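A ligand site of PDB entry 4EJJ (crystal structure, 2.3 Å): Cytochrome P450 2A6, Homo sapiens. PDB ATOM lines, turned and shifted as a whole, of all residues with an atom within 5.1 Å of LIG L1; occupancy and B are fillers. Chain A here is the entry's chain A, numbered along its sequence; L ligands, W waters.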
ATOM      1  N   LEU A  69      29.902  32.983 -13.251  1.00  0.00           N
ATOM      2  CA  LEU A  69      29.153  32.355 -14.316  1.00  0.00           C
ATOM      3  C   LEU A  69      29.524  32.871 -15.751  1.00  0.00           C
ATOM      4  O   LEU A  69      29.352  32.150 -16.740  1.00  0.00           O
ATOM      5  CB  LEU A  69      27.640  32.411 -14.028  1.00  0.00           C
ATOM      6  CG  LEU A  69      26.996  31.297 -13.200  1.00  0.00           C
ATOM      7  CD1 LEU A  69      27.699  30.954 -11.815  1.00  0.00           C
ATOM      8  CD2 LEU A  69      25.554  31.665 -12.979  1.00  0.00           C
ATOM      9  N   ARG A  79      25.850  21.294 -14.360  1.00  0.00           N
ATOM     10  CA  ARG A  79      24.487  21.343 -13.751  1.00  0.00           C
ATOM     11  C   ARG A  79      24.499  20.630 -12.403  1.00  0.00           C
ATOM     12  O   ARG A  79      24.902  19.506 -12.312  1.00  0.00           O
ATOM     13  CB  ARG A  79      23.440  20.664 -14.640  1.00  0.00           C
ATOM     14  CG  ARG A  79      21.997  20.562 -14.078  1.00  0.00           C
ATOM     15  CD  ARG A  79      21.404  21.970 -13.698  1.00  0.00           C
ATOM     16  NE  ARG A  79      21.090  22.802 -14.863  1.00  0.00           N
ATOM     17  CZ  ARG A  79      21.197  24.125 -14.917  1.00  0.00           C
ATOM     18  NH1 ARG A  79      21.632  24.843 -13.868  1.00  0.00           N
ATOM     19  NH2 ARG A  79      20.848  24.716 -16.037  1.00  0.00           N
ATOM     20  N   VAL A  94      17.371  17.848 -21.105  1.00  0.00           N
ATOM     21  CA  VAL A  94      18.235  18.980 -21.282  1.00  0.00           C
ATOM     22  C   VAL A  94      18.591  19.665 -19.927  1.00  0.00           C
ATOM     23  O   VAL A  94      19.769  19.815 -19.616  1.00  0.00           O
ATOM     24  CB  VAL A  94      17.730  19.897 -22.441  1.00  0.00           C
ATOM     25  CG1 VAL A  94      16.500  20.737 -22.062  1.00  0.00           C
ATOM     26  CG2 VAL A  94      18.843  20.737 -23.001  1.00  0.00           C
ATOM     27  N   VAL A  95      17.611  19.932 -19.068  1.00  0.00           N
ATOM     28  CA  VAL A  95      17.850  20.722 -17.864  1.00  0.00           C
ATOM     29  C   VAL A  95      18.848  20.081 -16.843  1.00  0.00           C
ATOM     30  O   VAL A  95      19.801  20.730 -16.445  1.00  0.00           O
ATOM     31  CB  VAL A  95      16.486  21.097 -17.185  1.00  0.00           C
ATOM     32  CG1 VAL A  95      16.683  21.815 -15.896  1.00  0.00           C
ATOM     33  CG2 VAL A  95      15.648  21.876 -18.153  1.00  0.00           C
ATOM     34  N   ARG A 106      21.016  20.469 -25.483  1.00  0.00           N
ATOM     35  CA  ARG A 106      20.885  21.918 -25.612  1.00  0.00           C
ATOM     36  C   ARG A 106      21.036  22.421 -27.044  1.00  0.00           C
ATOM     37  O   ARG A 106      20.172  23.101 -27.527  1.00  0.00           O
ATOM     38  CB  ARG A 106      21.822  22.646 -24.663  1.00  0.00           C
ATOM     39  CG  ARG A 106      21.745  24.174 -24.703  1.00  0.00           C
ATOM     40  CD  ARG A 106      22.640  24.733 -23.591  1.00  0.00           C
ATOM     41  NE  ARG A 106      22.756  26.146 -23.640  1.00  0.00           N
ATOM     42  CZ  ARG A 106      22.198  26.990 -22.783  1.00  0.00           C
ATOM     43  NH1 ARG A 106      21.482  26.550 -21.721  1.00  0.00           N
ATOM     44  NH2 ARG A 106      22.395  28.259 -22.967  1.00  0.00           N
ATOM     45  N   LEU A 113      13.626  24.553 -31.298  1.00  0.00           N
ATOM     46  CA  LEU A 113      12.799  25.704 -30.944  1.00  0.00           C
ATOM     47  C   LEU A 113      12.779  26.807 -32.050  1.00  0.00           C
ATOM     48  O   LEU A 113      11.702  27.374 -32.402  1.00  0.00           O
ATOM     49  CB  LEU A 113      13.253  26.283 -29.611  1.00  0.00           C
ATOM     50  CG  LEU A 113      12.457  26.035 -28.312  1.00  0.00           C
ATOM     51  CD1 LEU A 113      11.634  24.746 -28.253  1.00  0.00           C
ATOM     52  CD2 LEU A 113      13.383  26.095 -27.104  1.00  0.00           C
ATOM     53  N   ILE A 160       3.995  27.285 -25.911  1.00  0.00           N
ATOM     54  CA  ILE A 160       4.983  26.208 -25.916  1.00  0.00           C
ATOM     55  C   ILE A 160       4.373  24.831 -26.258  1.00  0.00           C
ATOM     56  O   ILE A 160       5.008  24.017 -26.912  1.00  0.00           O
ATOM     57  CB  ILE A 160       5.783  26.091 -24.546  1.00  0.00           C
ATOM     58  CG1 ILE A 160       6.837  25.006 -24.607  1.00  0.00           C
ATOM     59  CG2 ILE A 160       4.848  25.710 -23.428  1.00  0.00           C
ATOM     60  CD1 ILE A 160       7.957  25.336 -25.563  1.00  0.00           C
ATOM     61  N   ASN A 275      10.701  19.048 -19.507  1.00  0.00           N
ATOM     62  CA  ASN A 275      11.415  20.308 -19.206  1.00  0.00           C
ATOM     63  C   ASN A 275      10.791  21.514 -19.901  1.00  0.00           C
ATOM     64  O   ASN A 275      10.574  22.549 -19.260  1.00  0.00           O
ATOM     65  CB  ASN A 275      12.889  20.225 -19.671  1.00  0.00           C
ATOM     66  CG  ASN A 275      13.725  19.194 -18.885  1.00  0.00           C
ATOM     67  OD1 ASN A 275      14.723  18.717 -19.391  1.00  0.00           O
ATOM     68  ND2 ASN A 275      13.327  18.884 -17.637  1.00  0.00           N
ATOM     69  N   LEU A 276      10.519  21.395 -21.225  1.00  0.00           N
ATOM     70  CA  LEU A 276      10.061  22.519 -22.018  1.00  0.00           C
ATOM     71  C   LEU A 276       8.623  22.876 -21.700  1.00  0.00           C
ATOM     72  O   LEU A 276       8.266  24.053 -21.602  1.00  0.00           O
ATOM     73  CB  LEU A 276      10.222  22.249 -23.528  1.00  0.00           C
ATOM     74  CG  LEU A 276      11.690  22.153 -23.927  1.00  0.00           C
ATOM     75  CD1 LEU A 276      11.930  21.578 -25.365  1.00  0.00           C
ATOM     76  CD2 LEU A 276      12.167  23.547 -23.754  1.00  0.00           C
ATOM     77  N   GLY A 279       8.950  24.290 -18.116  1.00  0.00           N
ATOM     78  CA  GLY A 279       9.683  25.569 -18.153  1.00  0.00           C
ATOM     79  C   GLY A 279       8.935  26.624 -18.964  1.00  0.00           C
ATOM     80  O   GLY A 279       8.859  27.832 -18.619  1.00  0.00           O
ATOM     81  N   GLY A 280       8.305  26.140 -20.025  1.00  0.00           N
ATOM     82  CA  GLY A 280       7.595  27.003 -20.944  1.00  0.00           C
ATOM     83  C   GLY A 280       6.271  27.466 -20.426  1.00  0.00           C
ATOM     84  O   GLY A 280       5.716  28.345 -21.021  1.00  0.00           O
ATOM     85  N   THR A 283       6.966  29.546 -15.192  1.00  0.00           N
ATOM     86  CA  THR A 283       7.655  30.795 -14.865  1.00  0.00           C
ATOM     87  C   THR A 283       7.020  32.061 -15.492  1.00  0.00           C
ATOM     88  O   THR A 283       6.772  33.037 -14.780  1.00  0.00           O
ATOM     89  CB  THR A 283       9.165  30.747 -15.176  1.00  0.00           C
ATOM     90  OG1 THR A 283       9.391  29.876 -16.276  1.00  0.00           O
ATOM     91  CG2 THR A 283       9.886  30.157 -14.112  1.00  0.00           C
ATOM     92  N   VAL A 284       6.763  32.056 -16.805  1.00  0.00           N
ATOM     93  CA  VAL A 284       6.037  33.145 -17.460  1.00  0.00           C
ATOM     94  C   VAL A 284       4.679  33.382 -16.808  1.00  0.00           C
ATOM     95  O   VAL A 284       4.303  34.494 -16.463  1.00  0.00           O
ATOM     96  CB  VAL A 284       5.823  32.925 -18.971  1.00  0.00           C
ATOM     97  CG1 VAL A 284       4.882  34.008 -19.512  1.00  0.00           C
ATOM     98  CG2 VAL A 284       7.157  32.961 -19.724  1.00  0.00           C
ATOM     99  N   THR A 287       4.988  34.997 -13.523  1.00  0.00           N
ATOM    100  CA  THR A 287       5.431  36.390 -13.720  1.00  0.00           C
ATOM    101  C   THR A 287       4.256  37.309 -14.093  1.00  0.00           C
ATOM    102  O   THR A 287       4.121  38.407 -13.579  1.00  0.00           O
ATOM    103  CB  THR A 287       6.519  36.523 -14.777  1.00  0.00           C
ATOM    104  OG1 THR A 287       7.565  35.647 -14.446  1.00  0.00           O
ATOM    105  CG2 THR A 287       7.044  37.870 -14.783  1.00  0.00           C
ATOM    106  N   GLN A 338       9.761  41.468 -13.428  1.00  0.00           N
ATOM    107  CA  GLN A 338      10.749  40.402 -13.363  1.00  0.00           C
ATOM    108  C   GLN A 338      11.752  40.576 -12.224  1.00  0.00           C
ATOM    109  O   GLN A 338      11.946  39.650 -11.439  1.00  0.00           O
ATOM    110  CB  GLN A 338      11.484  40.197 -14.663  1.00  0.00           C
ATOM    111  CG  GLN A 338      10.597  39.672 -15.815  1.00  0.00           C
ATOM    112  CD  GLN A 338      11.422  38.956 -16.823  1.00  0.00           C
ATOM    113  OE1 GLN A 338      11.831  39.507 -17.814  1.00  0.00           O
ATOM    114  NE2 GLN A 338      11.687  37.705 -16.572  1.00  0.00           N
ATOM    115  N   VAL A 343      11.403  35.372  -9.575  1.00  0.00           N
ATOM    116  CA  VAL A 343      10.585  34.166  -9.621  1.00  0.00           C
ATOM    117  C   VAL A 343      11.404  32.896  -9.342  1.00  0.00           C
ATOM    118  O   VAL A 343      10.888  31.988  -8.705  1.00  0.00           O
ATOM    119  CB  VAL A 343       9.773  34.099 -10.962  1.00  0.00           C
ATOM    120  CG1 VAL A 343       9.013  32.788 -11.131  1.00  0.00           C
ATOM    121  CG2 VAL A 343       8.772  35.286 -11.067  1.00  0.00           C
ATOM    122  N   ILE A 344      12.642  32.869  -9.841  1.00  0.00           N
ATOM    123  CA  ILE A 344      13.628  31.807  -9.528  1.00  0.00           C
ATOM    124  C   ILE A 344      14.855  32.371  -8.760  1.00  0.00           C
ATOM    125  O   ILE A 344      15.949  32.551  -9.342  1.00  0.00           O
ATOM    126  CB  ILE A 344      14.071  30.988 -10.765  1.00  0.00           C
ATOM    127  CG1 ILE A 344      12.888  30.660 -11.693  1.00  0.00           C
ATOM    128  CG2 ILE A 344      14.868  29.744 -10.346  1.00  0.00           C
ATOM    129  CD1 ILE A 344      12.026  29.532 -11.299  1.00  0.00           C
ATOM    130  N   SER A 347      18.474  30.595  -8.696  1.00  0.00           N
ATOM    131  CA  SER A 347      18.669  29.928  -9.960  1.00  0.00           C
ATOM    132  C   SER A 347      18.323  28.349  -9.900  1.00  0.00           C
ATOM    133  O   SER A 347      17.603  27.877  -9.026  1.00  0.00           O
ATOM    134  CB  SER A 347      20.078  30.247 -10.493  1.00  0.00           C
ATOM    135  OG  SER A 347      20.134  29.983 -11.851  1.00  0.00           O
ATOM    136  N   LEU A 348      18.808  27.575 -10.862  1.00  0.00           N
ATOM    137  CA  LEU A 348      19.014  26.130 -10.689  1.00  0.00           C
ATOM    138  C   LEU A 348      20.497  25.965 -10.407  1.00  0.00           C
ATOM    139  O   LEU A 348      21.338  26.693 -10.985  1.00  0.00           O
ATOM    140  CB  LEU A 348      18.721  25.393 -11.954  1.00  0.00           C
ATOM    141  CG  LEU A 348      17.309  25.205 -12.409  1.00  0.00           C
ATOM    142  CD1 LEU A 348      16.381  26.517 -12.482  1.00  0.00           C
ATOM    143  CD2 LEU A 348      17.501  24.563 -13.805  1.00  0.00           C
ATOM    144  N   ARG A 350      24.279  25.144 -10.255  1.00  0.00           N
ATOM    145  CA  ARG A 350      25.432  24.823 -11.074  1.00  0.00           C
ATOM    146  C   ARG A 350      26.382  23.871 -10.371  1.00  0.00           C
ATOM    147  O   ARG A 350      26.213  23.569  -9.239  1.00  0.00           O
ATOM    148  CB  ARG A 350      26.165  26.072 -11.519  1.00  0.00           C
ATOM    149  CG  ARG A 350      25.385  26.984 -12.393  1.00  0.00           C
ATOM    150  CD  ARG A 350      25.050  26.379 -13.698  1.00  0.00           C
ATOM    151  NE  ARG A 350      24.586  27.363 -14.640  1.00  0.00           N
ATOM    152  CZ  ARG A 350      25.351  28.152 -15.352  1.00  0.00           C
ATOM    153  NH1 ARG A 350      26.638  28.078 -15.304  1.00  0.00           N
ATOM    154  NH2 ARG A 350      24.812  29.022 -16.132  1.00  0.00           N
ATOM    155  N   LEU A 373      20.459  34.582  -7.667  1.00  0.00           N
ATOM    156  CA  LEU A 373      19.950  35.539  -8.639  1.00  0.00           C
ATOM    157  C   LEU A 373      19.146  36.672  -7.960  1.00  0.00           C
ATOM    158  O   LEU A 373      19.261  37.858  -8.354  1.00  0.00           O
ATOM    159  CB  LEU A 373      19.080  34.847  -9.676  1.00  0.00           C
ATOM    160  CG  LEU A 373      19.685  33.728 -10.539  1.00  0.00           C
ATOM    161  CD1 LEU A 373      18.696  33.342 -11.624  1.00  0.00           C
ATOM    162  CD2 LEU A 373      20.976  34.248 -11.186  1.00  0.00           C
ATOM    163  N   PRO A 409      17.250  37.718 -14.330  1.00  0.00           N
ATOM    164  CA  PRO A 409      16.252  36.744 -13.912  1.00  0.00           C
ATOM    165  C   PRO A 409      16.376  35.418 -14.686  1.00  0.00           C
ATOM    166  O   PRO A 409      15.851  34.396 -14.205  1.00  0.00           O
ATOM    167  CB  PRO A 409      14.916  37.419 -14.289  1.00  0.00           C
ATOM    168  CG  PRO A 409      15.272  38.197 -15.552  1.00  0.00           C
ATOM    169  CD  PRO A 409      16.650  38.793 -15.148  1.00  0.00           C
ATOM    170  N   PHE A 410      17.017  35.433 -15.858  1.00  0.00           N
ATOM    171  CA  PHE A 410      17.164  34.209 -16.672  1.00  0.00           C
ATOM    172  C   PHE A 410      18.540  33.571 -16.370  1.00  0.00           C
ATOM    173  O   PHE A 410      18.960  32.635 -17.045  1.00  0.00           O
ATOM    174  CB  PHE A 410      17.020  34.533 -18.176  1.00  0.00           C
ATOM    175  CG  PHE A 410      15.620  35.065 -18.572  1.00  0.00           C
ATOM    176  CD1 PHE A 410      14.528  34.195 -18.691  1.00  0.00           C
ATOM    177  CD2 PHE A 410      15.429  36.428 -18.787  1.00  0.00           C
ATOM    178  CE1 PHE A 410      13.243  34.650 -19.057  1.00  0.00           C
ATOM    179  CE2 PHE A 410      14.176  36.952 -19.153  1.00  0.00           C
ATOM    180  CZ  PHE A 410      13.047  36.049 -19.302  1.00  0.00           C
ATOM    181  N   SER A 411      19.253  34.115 -15.363  1.00  0.00           N
ATOM    182  CA  SER A 411      20.641  33.780 -15.142  1.00  0.00           C
ATOM    183  C   SER A 411      21.545  34.216 -16.376  1.00  0.00           C
ATOM    184  O   SER A 411      21.137  35.124 -17.116  1.00  0.00           O
ATOM    185  CB  SER A 411      20.752  32.334 -14.732  1.00  0.00           C
ATOM    186  OG  SER A 411      22.020  31.910 -14.435  1.00  0.00           O
ATOM    187  N   ILE A 412      22.726  33.583 -16.556  1.00  0.00           N
ATOM    188  CA  ILE A 412      23.845  34.015 -17.455  1.00  0.00           C
ATOM    189  C   ILE A 412      24.891  32.912 -17.469  1.00  0.00           C
ATOM    190  O   ILE A 412      24.901  31.998 -16.597  1.00  0.00           O
ATOM    191  CB  ILE A 412      24.561  35.422 -17.037  1.00  0.00           C
ATOM    192  CG1 ILE A 412      25.151  35.361 -15.591  1.00  0.00           C
ATOM    193  CG2 ILE A 412      23.619  36.640 -17.302  1.00  0.00           C
ATOM    194  CD1 ILE A 412      25.720  36.712 -14.989  1.00  0.00           C
ATOM    195  N   ARG A 415      24.936  27.693 -19.324  1.00  0.00           N
ATOM    196  CA  ARG A 415      23.720  26.962 -19.105  1.00  0.00           C
ATOM    197  C   ARG A 415      22.602  27.931 -18.666  1.00  0.00           C
ATOM    198  O   ARG A 415      21.690  27.553 -17.924  1.00  0.00           O
ATOM    199  CB  ARG A 415      23.937  25.809 -18.128  1.00  0.00           C
ATOM    200  CG  ARG A 415      25.093  24.850 -18.604  1.00  0.00           C
ATOM    201  CD  ARG A 415      24.697  23.777 -19.595  1.00  0.00           C
ATOM    202  NE  ARG A 415      23.496  23.046 -19.181  1.00  0.00           N
ATOM    203  CZ  ARG A 415      23.447  21.863 -18.566  1.00  0.00           C
ATOM    204  NH1 ARG A 415      22.250  21.361 -18.233  1.00  0.00           N
ATOM    205  NH2 ARG A 415      24.569  21.201 -18.256  1.00  0.00           N
ATOM    206  N   ASN A 416      22.689  29.162 -19.162  1.00  0.00           N
ATOM    207  CA  ASN A 416      21.649  30.186 -18.879  1.00  0.00           C
ATOM    208  C   ASN A 416      20.283  29.776 -19.509  1.00  0.00           C
ATOM    209  O   ASN A 416      20.254  28.886 -20.353  1.00  0.00           O
ATOM    210  CB  ASN A 416      22.127  31.561 -19.365  1.00  0.00           C
ATOM    211  CG  ASN A 416      22.104  31.709 -20.917  1.00  0.00           C
ATOM    212  OD1 ASN A 416      22.379  30.757 -21.689  1.00  0.00           O
ATOM    213  ND2 ASN A 416      21.864  32.915 -21.356  1.00  0.00           N
ATOM    214  N   CYS A 417      19.154  30.366 -19.084  1.00  0.00           N
ATOM    215  CA  CYS A 417      17.843  29.983 -19.654  1.00  0.00           C
ATOM    216  C   CYS A 417      17.785  30.154 -21.187  1.00  0.00           C
ATOM    217  O   CYS A 417      17.939  31.280 -21.662  1.00  0.00           O
ATOM    218  CB  CYS A 417      16.676  30.792 -19.044  1.00  0.00           C
ATOM    219  SG  CYS A 417      15.030  30.331 -19.853  1.00  0.00           S
ATOM    220  N   PHE A 418      17.612  29.085 -21.961  1.00  0.00           N
ATOM    221  CA  PHE A 418      17.393  29.291 -23.437  1.00  0.00           C
ATOM    222  C   PHE A 418      15.933  29.564 -23.905  1.00  0.00           C
ATOM    223  O   PHE A 418      15.597  29.672 -25.086  1.00  0.00           O
ATOM    224  CB  PHE A 418      18.183  28.268 -24.310  1.00  0.00           C
ATOM    225  CG  PHE A 418      17.741  26.868 -24.173  1.00  0.00           C
ATOM    226  CD1 PHE A 418      16.538  26.458 -24.745  1.00  0.00           C
ATOM    227  CD2 PHE A 418      18.542  25.917 -23.520  1.00  0.00           C
ATOM    228  CE1 PHE A 418      16.124  25.137 -24.622  1.00  0.00           C
ATOM    229  CE2 PHE A 418      18.108  24.588 -23.392  1.00  0.00           C
ATOM    230  CZ  PHE A 418      16.902  24.216 -23.901  1.00  0.00           C
ATOM    231  N   GLY A 419      15.034  29.648 -22.933  1.00  0.00           N
ATOM    232  CA  GLY A 419      13.702  30.063 -23.180  1.00  0.00           C
ATOM    233  C   GLY A 419      13.526  31.562 -23.038  1.00  0.00           C
ATOM    234  O   GLY A 419      12.456  32.055 -23.308  1.00  0.00           O
ATOM    235  N   GLU A 420      14.572  32.266 -22.601  1.00  0.00           N
ATOM    236  CA  GLU A 420      14.589  33.733 -22.540  1.00  0.00           C
ATOM    237  C   GLU A 420      13.882  34.396 -23.760  1.00  0.00           C
ATOM    238  O   GLU A 420      13.067  35.281 -23.596  1.00  0.00           O
ATOM    239  CB  GLU A 420      16.038  34.309 -22.417  1.00  0.00           C
ATOM    240  CG  GLU A 420      15.985  35.883 -22.347  1.00  0.00           C
ATOM    241  CD  GLU A 420      17.298  36.667 -21.955  1.00  0.00           C
ATOM    242  OE1 GLU A 420      17.257  37.925 -21.980  1.00  0.00           O
ATOM    243  OE2 GLU A 420      18.329  36.068 -21.653  1.00  0.00           O
ATOM    244  N   LEU A 422      11.751  33.308 -26.281  1.00  0.00           N
ATOM    245  CA  LEU A 422      10.294  33.054 -26.082  1.00  0.00           C
ATOM    246  C   LEU A 422       9.620  33.847 -24.942  1.00  0.00           C
ATOM    247  O   LEU A 422       8.573  34.459 -25.131  1.00  0.00           O
ATOM    248  CB  LEU A 422      10.021  31.567 -25.886  1.00  0.00           C
ATOM    249  CG  LEU A 422       8.535  31.227 -25.932  1.00  0.00           C
ATOM    250  CD1 LEU A 422       7.832  31.857 -27.195  1.00  0.00           C
ATOM    251  CD2 LEU A 422       8.291  29.740 -25.863  1.00  0.00           C
ATOM    252  N   ALA A 423      10.228  33.833 -23.758  1.00  0.00           N
ATOM    253  CA  ALA A 423       9.614  34.433 -22.594  1.00  0.00           C
ATOM    254  C   ALA A 423       9.395  35.915 -22.733  1.00  0.00           C
ATOM    255  O   ALA A 423       8.396  36.413 -22.286  1.00  0.00           O
ATOM    256  CB  ALA A 423      10.443  34.146 -21.328  1.00  0.00           C
ATOM    257  N   LEU A 427       5.840  37.759 -22.551  1.00  0.00           N
ATOM    258  CA  LEU A 427       5.638  38.797 -21.580  1.00  0.00           C
ATOM    259  C   LEU A 427       5.290  40.147 -22.193  1.00  0.00           C
ATOM    260  O   LEU A 427       4.377  40.786 -21.717  1.00  0.00           O
ATOM    261  CB  LEU A 427       6.828  38.907 -20.596  1.00  0.00           C
ATOM    262  CG  LEU A 427       7.006  37.761 -19.576  1.00  0.00           C
ATOM    263  CD1 LEU A 427       8.245  37.994 -18.784  1.00  0.00           C
ATOM    264  CD2 LEU A 427       5.832  37.645 -18.651  1.00  0.00           C
HETATM  265  C1  LIG L   1      16.967  27.352 -17.288  1.00  0.00           C
HETATM  266  C2  LIG L   1      14.537  31.097 -15.443  1.00  0.00           C
HETATM  267  C3  LIG L   1      11.424  30.710 -19.127  1.00  0.00           C
HETATM  268  C4  LIG L   1      13.306  26.558 -20.515  1.00  0.00           C
HETATM  269  C5  LIG L   1      16.633  28.414 -16.467  1.00  0.00           C
HETATM  270  C6  LIG L   1      17.401  28.945 -15.358  1.00  0.00           C
HETATM  271  C7  LIG L   1      16.735  30.009 -14.891  1.00  0.00           C
HETATM  272  C8  LIG L   1      15.529  30.169 -15.643  1.00  0.00           C
HETATM  273  C9  LIG L   1      17.069  30.940 -13.712  1.00  0.00           C
HETATM  274  C10 LIG L   1      18.761  28.359 -14.902  1.00  0.00           C
HETATM  275  C11 LIG L   1      19.816  28.875 -15.880  1.00  0.00           C
HETATM  276  C12 LIG L   1      21.207  28.609 -15.324  1.00  0.00           C
HETATM  277  O1  LIG L   1      22.076  29.502 -15.346  1.00  0.00           O
HETATM  278  O2  LIG L   1      21.424  27.492 -14.844  1.00  0.00           O
HETATM  279  C13 LIG L   1      13.459  31.396 -16.306  1.00  0.00           C
HETATM  280  C14 LIG L   1      12.560  32.466 -16.214  1.00  0.00           C
HETATM  281  C15 LIG L   1      11.715  32.329 -17.243  1.00  0.00           C
HETATM  282  C16 LIG L   1      12.058  31.161 -17.995  1.00  0.00           C
HETATM  283  C17 LIG L   1      12.539  33.641 -15.181  1.00  0.00           C
HETATM  284  C18 LIG L   1      10.527  33.271 -17.662  1.00  0.00           C
HETATM  285  C19 LIG L   1       9.959  34.132 -16.819  1.00  0.00           C
HETATM  286  C20 LIG L   1      11.625  29.581 -19.846  1.00  0.00           C
HETATM  287  C21 LIG L   1      10.882  29.076 -20.975  1.00  0.00           C
HETATM  288  C22 LIG L   1      11.394  27.902 -21.357  1.00  0.00           C
HETATM  289  C23 LIG L   1      12.472  27.621 -20.479  1.00  0.00           C
HETATM  290  C24 LIG L   1       9.660  29.741 -21.609  1.00  0.00           C
HETATM  291  C25 LIG L   1      10.853  27.041 -22.494  1.00  0.00           C
HETATM  292  C26 LIG L   1      11.146  27.283 -23.767  1.00  0.00           C
HETATM  293  C27 LIG L   1      14.476  26.367 -19.783  1.00  0.00           C
HETATM  294  C28 LIG L   1      15.399  25.268 -19.942  1.00  0.00           C
HETATM  295  C29 LIG L   1      16.577  25.516 -18.982  1.00  0.00           C
HETATM  296  C30 LIG L   1      16.214  26.759 -18.299  1.00  0.00           C
HETATM  297  C31 LIG L   1      15.240  24.090 -20.916  1.00  0.00           C
HETATM  298  C32 LIG L   1      17.821  24.665 -18.717  1.00  0.00           C
HETATM  299  C33 LIG L   1      19.090  25.294 -19.297  1.00  0.00           C
HETATM  300  C34 LIG L   1      20.199  24.279 -19.454  1.00  0.00           C
HETATM  301  O3  LIG L   1      20.944  24.287 -20.468  1.00  0.00           O
HETATM  302  O4  LIG L   1      20.356  23.471 -18.541  1.00  0.00           O
HETATM  303  N1  LIG L   1      15.536  29.195 -16.603  1.00  0.00           N
HETATM  304  N2  LIG L   1      13.110  30.635 -17.382  1.00  0.00           N
HETATM  305  N3  LIG L   1      12.584  28.679 -19.614  1.00  0.00           N
HETATM  306  N4  LIG L   1      15.015  27.224 -18.862  1.00  0.00           N
HETATM  307 FE1  LIG L   1      14.077  28.990 -18.150  1.00  0.00          FE
HETATM  308  N1  LG2 L   2      12.039  21.771 -15.485  1.00  0.00           N
HETATM  309  C1  LG2 L   2      12.038  23.003 -16.004  1.00  0.00           C
HETATM  310  C2  LG2 L   2      12.471  24.059 -15.209  1.00  0.00           C
HETATM  311  C3  LG2 L   2      12.906  23.871 -13.892  1.00  0.00           C
HETATM  312  C4  LG2 L   2      12.894  22.571 -13.406  1.00  0.00           C
HETATM  313  C5  LG2 L   2      12.457  21.537 -14.226  1.00  0.00           C
HETATM  314  N2  LG2 L   2      12.065  26.466 -14.952  1.00  0.00           N
HETATM  315  C6  LG2 L   2      12.374  25.381 -15.827  1.00  0.00           C
HETATM  316  C7  LG2 L   2      13.639  25.976 -16.398  1.00  0.00           C
HETATM  317  C8  LG2 L   2      13.162  27.385 -16.724  1.00  0.00           C
HETATM  318  C9  LG2 L   2      12.087  27.720 -15.707  1.00  0.00           C
HETATM  319  C10 LG2 L   2      11.804  26.394 -13.539  1.00  0.00           C
HETATM  320  O   HOH W   1      22.544  29.003 -12.487  1.00  0.00           O
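The side-chain sulfur (SG) of Cys 417 lies close to the backbone NH (N) of Gly 419, at 3.2 Å. SG of Cys 417 lies close to N of Glu 420 (3.4 Å). OD1 of Asn 416 lies within hydrogen-bond range of NH2 of Arg 106, 2.8 Å away. O of Val 94 lies within hydrogen-bond range of NH1 of Arg 415 (3.2 Å). O of Ile 412 sits at hydrogen-bond distance from NH2 of Arg 350 (3.0 Å). The side-chain hydroxyl of Thr 283 lies within hydrogen-bond range of the backbone carbonyl oxygen of Gly 279 (3.2 Å). The side-chain amide oxygen (OD1) of Asn 275 sits at hydrogen-bond distance from the backbone NH (N) of Val 95, 3.1 Å away. N of Val 94 lies within hydrogen-bond range of OD1 of Asn 275 (3.3 Å).
Water W1 lies within hydrogen-bond range of the side-chain hydroxyl (OG) of Ser 347, an oxygen (O1) of LIG L1, the backbone carbonyl oxygen (O) of Leu 348 and the guanidinium group (NE) of Arg 350.
An iron atom (FE1) of LIG L1 is bound by the side-chain sulfur (SG) of Cys 417 (2.4 Å). O1 of LIG L1 is in hydrogen-bond range of OG of Ser 411 (2.6 Å). The guanidinium group (NH1) of Arg 106 is in salt-bridge range of an oxygen (O3) of LIG L1, at 2.6 Å. An oxygen (O2) of LIG L1 lies within salt-bridge range of the guanidinium group (NH1) of Arg 79. O of Arg 415 lies close to O2 of LIG L1, at 3.1 Å. NH1 of Arg 415 is in salt-bridge range of O4 of LIG L1 (2.9 Å). NH2 of Arg 350 is in salt-bridge range of O1 of LIG L1 (2.9 Å).
O of Val 95 lies close to O4 of LIG L1 (3.5 Å). CG1 of Val 94 touches C31 of LIG L1 (3.8 Å). Leu 276 touches LIG L1 (CD2 to C26, 3.9 Å). O of Gly 279 touches C21 of LIG L1, at 3.3 Å. CA of Gly 280 touches C24 of LIG L1, at 3.5 Å. Thr 283 touches LIG L1 (OG1 to C16, 3.4 Å). N of Val 284 touches C19 of LIG L1, 3.8 Å away. OG1 of Thr 287 touches C19 of LIG L1, at 3.7 Å. Gln 338 touches LIG L1. Ser 347 touches LIG L1 (OG to C9, 3.7 Å). Leu 348 touches LIG L1. Leu 373 touches LIG L1 (CD1 to C9, 3.6 Å). O of Pro 409 touches C17 of LIG L1, at 3.5 Å. Phe 410 touches LIG L1 (CE1 to C15, 3.3 Å). O of Ile 412 touches O1 of LIG L1, 3.97 Å away. CA of Asn 416 touches O1 of LIG L1, 3.6 Å away. Phe 418 touches LIG L1 (CZ to C31, 3.4 Å). Gly 419 touches LIG L1 (CA to C22, 3.6 Å). Ala 423 touches LIG L1 (CB to C18, 3.8 Å).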
